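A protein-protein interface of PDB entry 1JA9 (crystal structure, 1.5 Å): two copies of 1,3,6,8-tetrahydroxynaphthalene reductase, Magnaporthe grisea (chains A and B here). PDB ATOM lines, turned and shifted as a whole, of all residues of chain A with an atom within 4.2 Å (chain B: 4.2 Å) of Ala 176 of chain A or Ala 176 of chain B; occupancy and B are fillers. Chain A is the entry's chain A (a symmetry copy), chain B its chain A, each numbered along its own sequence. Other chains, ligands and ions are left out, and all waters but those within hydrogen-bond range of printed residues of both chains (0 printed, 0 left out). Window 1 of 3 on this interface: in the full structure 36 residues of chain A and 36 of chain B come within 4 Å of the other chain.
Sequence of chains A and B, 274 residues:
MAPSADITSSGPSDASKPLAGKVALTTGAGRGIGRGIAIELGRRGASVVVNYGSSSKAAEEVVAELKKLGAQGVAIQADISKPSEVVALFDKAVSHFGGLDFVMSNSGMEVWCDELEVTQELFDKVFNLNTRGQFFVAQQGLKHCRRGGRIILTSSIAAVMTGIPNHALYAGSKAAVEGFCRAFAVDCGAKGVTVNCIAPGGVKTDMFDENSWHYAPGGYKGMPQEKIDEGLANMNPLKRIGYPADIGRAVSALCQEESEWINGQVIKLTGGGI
Of the 10 printed residues of chain B, 4 touch a printed residue of chain A.
Printed residues of chain B that touch a printed residue of chain A: Gly 172, Ala 175, Ala 176 and Phe 180.
Hydrophobic or aromatic side chains of chain B within 4 Å of the printed part of chain A: Ala 175, Ala 176 and Phe 180.
Of the 10 printed residues of chain A, 4 touch a printed residue of chain B.
Hydrophobic or aromatic side chains of chain A that line the printed part of chain B: Ala 175, Ala 176 and Phe 180.
Among the printed residues, 6 pairs touch across the chains.
Of chain B, only Gly 172 and Ala 176 come within 4 Å of Ala 176 of chain A.
Ala 176 of chain B touches just these residues of chain A: Gly 172 and Ala 176.
Of the printed residues of chain B, Ala 175 of chain A touches Ala 175.
Printed residues of chain A within 4 Å of Ala 175 of chain B: Ala 175.
Thr 131 of chain B touches none of the printed residues of chain A.
The nearest printed residue of chain B that does not touch Ala 176 of chain A is Ala 175 of chain B (4.2 Å).
Gly 172 of chain A touches Ala 176 of chain B, and with the chains exchanged Ala 176 of chain A touches Gly 172 of chain B.
Gly 172 of chain A touches Phe 180 of chain B, and with the chains exchanged Phe 180 of chain A touches Gly 172 of chain B.
Ala 175 of chain B touches its own counterpart, Ala 175 of chain A.
Ala 176 of chain A touches its own counterpart, Ala 176 of chain B.
10 positions are printed for both chains.
Of the 6 pairs that touch across the chains among the printed residues, 6 have their exchanged pair printed and touching as well.
Among the printed residues, pairs that only touch across the chains: Gly 172 of chain A with Ala 176 of chain B (3.3 Å), Gly 172 of chain A with Phe 180 of chain B (3.7 Å), Ala 175 of chain A with Ala 175 of chain B (3.5 Å), Ala 176 of chain A with Gly 172 of chain B (3.3 Å), Ala 176 of chain A with Ala 176 of chain B (3.9 Å) and Phe 180 of chain A with Gly 172 of chain B (3.7 Å).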
ATOM      1  N   THR A 131      -8.876 -31.432  13.653  1.00  0.00           N
ATOM      2  CA  THR A 131      -9.042 -31.443  12.223  1.00  0.00           C
ATOM      3  C   THR A 131      -7.879 -32.096  11.489  1.00  0.00           C
ATOM      4  O   THR A 131      -8.082 -33.083  10.788  1.00  0.00           O
ATOM      5  CB  THR A 131      -9.254 -29.991  11.714  1.00  0.00           C
ATOM      6  OG1 THR A 131     -10.296 -29.380  12.496  1.00  0.00           O
ATOM      7  CG2 THR A 131      -9.596 -29.970  10.233  1.00  0.00           C
ATOM      8  N   GLY A 172     -15.904 -24.902  14.075  1.00  0.00           N
ATOM      9  CA  GLY A 172     -15.204 -24.929  12.798  1.00  0.00           C
ATOM     10  C   GLY A 172     -14.324 -26.163  12.612  1.00  0.00           C
ATOM     11  O   GLY A 172     -14.268 -26.737  11.512  1.00  0.00           O
ATOM     12  N   SER A 173     -13.660 -26.582  13.690  1.00  0.00           N
ATOM     13  CA  SER A 173     -12.751 -27.735  13.593  1.00  0.00           C
ATOM     14  C   SER A 173     -13.554 -29.019  13.364  1.00  0.00           C
ATOM     15  O   SER A 173     -13.094 -29.929  12.690  1.00  0.00           O
ATOM     16  CB  SER A 173     -11.856 -27.847  14.834  1.00  0.00           C
ATOM     17  OG  SER A 173     -12.602 -28.209  15.975  1.00  0.00           O
ATOM     18  N   LYS A 174     -14.757 -29.082  13.903  1.00  0.00           N
ATOM     19  CA  LYS A 174     -15.592 -30.267  13.694  1.00  0.00           C
ATOM     20  C   LYS A 174     -16.285 -30.217  12.319  1.00  0.00           C
ATOM     21  O   LYS A 174     -16.343 -31.216  11.597  1.00  0.00           O
ATOM     22  CB  LYS A 174     -16.606 -30.376  14.820  1.00  0.00           C
ATOM     23  CG  LYS A 174     -15.976 -30.664  16.194  1.00  0.00           C
ATOM     24  CD  LYS A 174     -15.190 -31.972  16.152  1.00  0.00           C
ATOM     25  CE  LYS A 174     -15.104 -32.587  17.555  1.00  0.00           C
ATOM     26  NZ  LYS A 174     -14.447 -33.926  17.562  1.00  0.00           N
ATOM     27  N   ALA A 175     -16.801 -29.045  11.927  1.00  0.00           N
ATOM     28  CA  ALA A 175     -17.456 -28.931  10.613  1.00  0.00           C
ATOM     29  C   ALA A 175     -16.474 -29.352   9.499  1.00  0.00           C
ATOM     30  O   ALA A 175     -16.871 -29.986   8.521  1.00  0.00           O
ATOM     31  CB  ALA A 175     -17.942 -27.479  10.369  1.00  0.00           C
ATOM     32  N   ALA A 176     -15.191 -29.020   9.656  1.00  0.00           N
ATOM     33  CA  ALA A 176     -14.185 -29.365   8.635  1.00  0.00           C
ATOM     34  C   ALA A 176     -14.164 -30.858   8.311  1.00  0.00           C
ATOM     35  O   ALA A 176     -14.030 -31.258   7.168  1.00  0.00           O
ATOM     36  CB  ALA A 176     -12.807 -28.942   9.113  1.00  0.00           C
ATOM     37  N   VAL A 177     -14.312 -31.663   9.351  1.00  0.00           N
ATOM     38  CA  VAL A 177     -14.257 -33.118   9.240  1.00  0.00           C
ATOM     39  C   VAL A 177     -15.410 -33.695   8.422  1.00  0.00           C
ATOM     40  O   VAL A 177     -15.267 -34.742   7.770  1.00  0.00           O
ATOM     41  CB  VAL A 177     -14.163 -33.702  10.658  1.00  0.00           C
ATOM     42  CG1 VAL A 177     -14.478 -35.133  10.688  1.00  0.00           C
ATOM     43  CG2 VAL A 177     -12.763 -33.371  11.237  1.00  0.00           C
ATOM     44  N   GLU A 178     -16.538 -32.984   8.422  1.00  0.00           N
ATOM     45  CA  GLU A 178     -17.699 -33.393   7.635  1.00  0.00           C
ATOM     46  C   GLU A 178     -17.345 -33.266   6.132  1.00  0.00           C
ATOM     47  O   GLU A 178     -17.713 -34.121   5.314  1.00  0.00           O
ATOM     48  CB  GLU A 178     -18.916 -32.574   8.051  1.00  0.00           C
ATOM     49  CG  GLU A 178     -19.187 -32.787   9.525  1.00  0.00           C
ATOM     50  CD  GLU A 178     -20.436 -32.095  10.039  1.00  0.00           C
ATOM     51  OE1 GLU A 178     -20.709 -32.192  11.258  1.00  0.00           O
ATOM     52  OE2 GLU A 178     -21.155 -31.471   9.224  1.00  0.00           O
ATOM     53  N   GLY A 179     -16.572 -32.226   5.790  1.00  0.00           N
ATOM     54  CA  GLY A 179     -16.115 -32.057   4.418  1.00  0.00           C
ATOM     55  C   GLY A 179     -15.133 -33.180   4.092  1.00  0.00           C
ATOM     56  O   GLY A 179     -15.169 -33.731   3.005  1.00  0.00           O
ATOM     57  N   PHE A 180     -14.257 -33.535   5.034  1.00  0.00           N
ATOM     58  CA  PHE A 180     -13.305 -34.643   4.815  1.00  0.00           C
ATOM     59  C   PHE A 180     -14.053 -35.949   4.544  1.00  0.00           C
ATOM     60  O   PHE A 180     -13.628 -36.745   3.707  1.00  0.00           O
ATOM     61  CB  PHE A 180     -12.419 -34.889   6.050  1.00  0.00           C
ATOM     62  CG  PHE A 180     -11.411 -33.797   6.332  1.00  0.00           C
ATOM     63  CD1 PHE A 180     -11.019 -32.895   5.353  1.00  0.00           C
ATOM     64  CD2 PHE A 180     -10.842 -33.698   7.597  1.00  0.00           C
ATOM     65  CE1 PHE A 180     -10.051 -31.893   5.652  1.00  0.00           C
ATOM     66  CE2 PHE A 180      -9.881 -32.704   7.902  1.00  0.00           C
ATOM     67  CZ  PHE A 180      -9.495 -31.811   6.931  1.00  0.00           C
ATOM     68  N   THR B 131      -9.035 -21.178   5.939  1.00  0.00           N
ATOM     69  CA  THR B 131      -9.749 -21.322   7.182  1.00  0.00           C
ATOM     70  C   THR B 131      -9.256 -20.377   8.269  1.00  0.00           C
ATOM     71  O   THR B 131     -10.032 -19.562   8.761  1.00  0.00           O
ATOM     72  CB  THR B 131      -9.657 -22.795   7.665  1.00  0.00           C
ATOM     73  OG1 THR B 131     -10.041 -23.657   6.578  1.00  0.00           O
ATOM     74  CG2 THR B 131     -10.531 -23.030   8.886  1.00  0.00           C
ATOM     75  N   GLY B 172     -12.757 -29.602   3.221  1.00  0.00           N
ATOM     76  CA  GLY B 172     -12.673 -29.437   4.666  1.00  0.00           C
ATOM     77  C   GLY B 172     -12.396 -27.999   5.099  1.00  0.00           C
ATOM     78  O   GLY B 172     -12.971 -27.517   6.088  1.00  0.00           O
ATOM     79  N   SER B 173     -11.536 -27.312   4.347  1.00  0.00           N
ATOM     80  CA  SER B 173     -11.172 -25.934   4.715  1.00  0.00           C
ATOM     81  C   SER B 173     -12.372 -25.003   4.517  1.00  0.00           C
ATOM     82  O   SER B 173     -12.543 -24.043   5.252  1.00  0.00           O
ATOM     83  CB  SER B 173      -9.949 -25.449   3.927  1.00  0.00           C
ATOM     84  OG  SER B 173     -10.254 -25.272   2.561  1.00  0.00           O
ATOM     85  N   LYS B 174     -13.210 -25.300   3.541  1.00  0.00           N
ATOM     86  CA  LYS B 174     -14.397 -24.471   3.319  1.00  0.00           C
ATOM     87  C   LYS B 174     -15.521 -24.841   4.306  1.00  0.00           C
ATOM     88  O   LYS B 174     -16.183 -23.969   4.874  1.00  0.00           O
ATOM     89  CB  LYS B 174     -14.856 -24.622   1.878  1.00  0.00           C
ATOM     90  CG  LYS B 174     -13.865 -24.048   0.850  1.00  0.00           C
ATOM     91  CD  LYS B 174     -13.635 -22.562   1.110  1.00  0.00           C
ATOM     92  CE  LYS B 174     -13.206 -21.856  -0.184  1.00  0.00           C
ATOM     93  NZ  LYS B 174     -13.078 -20.377  -0.023  1.00  0.00           N
ATOM     94  N   ALA B 175     -15.735 -26.142   4.541  1.00  0.00           N
ATOM     95  CA  ALA B 175     -16.780 -26.556   5.493  1.00  0.00           C
ATOM     96  C   ALA B 175     -16.519 -25.916   6.872  1.00  0.00           C
ATOM     97  O   ALA B 175     -17.455 -25.516   7.565  1.00  0.00           O
ATOM     98  CB  ALA B 175     -16.820 -28.100   5.624  1.00  0.00           C
ATOM     99  N   ALA B 176     -15.247 -25.797   7.260  1.00  0.00           N
ATOM    100  CA  ALA B 176     -14.902 -25.215   8.570  1.00  0.00           C
ATOM    101  C   ALA B 176     -15.502 -23.823   8.770  1.00  0.00           C
ATOM    102  O   ALA B 176     -15.971 -23.482   9.842  1.00  0.00           O
ATOM    103  CB  ALA B 176     -13.393 -25.128   8.709  1.00  0.00           C
ATOM    104  N   VAL B 177     -15.479 -23.040   7.704  1.00  0.00           N
ATOM    105  CA  VAL B 177     -15.953 -21.659   7.725  1.00  0.00           C
ATOM    106  C   VAL B 177     -17.455 -21.550   7.977  1.00  0.00           C
ATOM    107  O   VAL B 177     -17.934 -20.562   8.556  1.00  0.00           O
ATOM    108  CB  VAL B 177     -15.501 -20.978   6.424  1.00  0.00           C
ATOM    109  CG1 VAL B 177     -16.227 -19.731   6.171  1.00  0.00           C
ATOM    110  CG2 VAL B 177     -13.962 -20.792   6.473  1.00  0.00           C
ATOM    111  N   GLU B 178     -18.189 -22.589   7.579  1.00  0.00           N
ATOM    112  CA  GLU B 178     -19.631 -22.639   7.810  1.00  0.00           C
ATOM    113  C   GLU B 178     -19.882 -22.748   9.334  1.00  0.00           C
ATOM    114  O   GLU B 178     -20.802 -22.119   9.877  1.00  0.00           O
ATOM    115  CB  GLU B 178     -20.242 -23.780   7.003  1.00  0.00           C
ATOM    116  CG  GLU B 178     -19.960 -23.565   5.531  1.00  0.00           C
ATOM    117  CD  GLU B 178     -20.600 -24.590   4.614  1.00  0.00           C
ATOM    118  OE1 GLU B 178     -20.382 -24.502   3.383  1.00  0.00           O
ATOM    119  OE2 GLU B 178     -21.336 -25.470   5.118  1.00  0.00           O
ATOM    120  N   GLY B 179     -19.015 -23.499  10.027  1.00  0.00           N
ATOM    121  CA  GLY B 179     -19.112 -23.604  11.475  1.00  0.00           C
ATOM    122  C   GLY B 179     -18.767 -22.247  12.086  1.00  0.00           C
ATOM    123  O   GLY B 179     -19.410 -21.816  13.027  1.00  0.00           O
ATOM    124  N   PHE B 180     -17.758 -21.561  11.545  1.00  0.00           N
ATOM    125  CA  PHE B 180     -17.392 -20.220  12.046  1.00  0.00           C
ATOM    126  C   PHE B 180     -18.568 -19.253  11.907  1.00  0.00           C
ATOM    127  O   PHE B 180     -18.796 -18.422  12.785  1.00  0.00           O
ATOM    128  CB  PHE B 180     -16.222 -19.612  11.250  1.00  0.00           C
ATOM    129  CG  PHE B 180     -14.889 -20.291  11.469  1.00  0.00           C
ATOM    130  CD1 PHE B 180     -14.645 -21.081  12.583  1.00  0.00           C
ATOM    131  CD2 PHE B 180     -13.866 -20.110  10.543  1.00  0.00           C
ATOM    132  CE1 PHE B 180     -13.368 -21.687  12.764  1.00  0.00           C
ATOM    133  CE2 PHE B 180     -12.595 -20.710  10.715  1.00  0.00           C
ATOM    134  CZ  PHE B 180     -12.357 -21.493  11.820  1.00  0.00           C
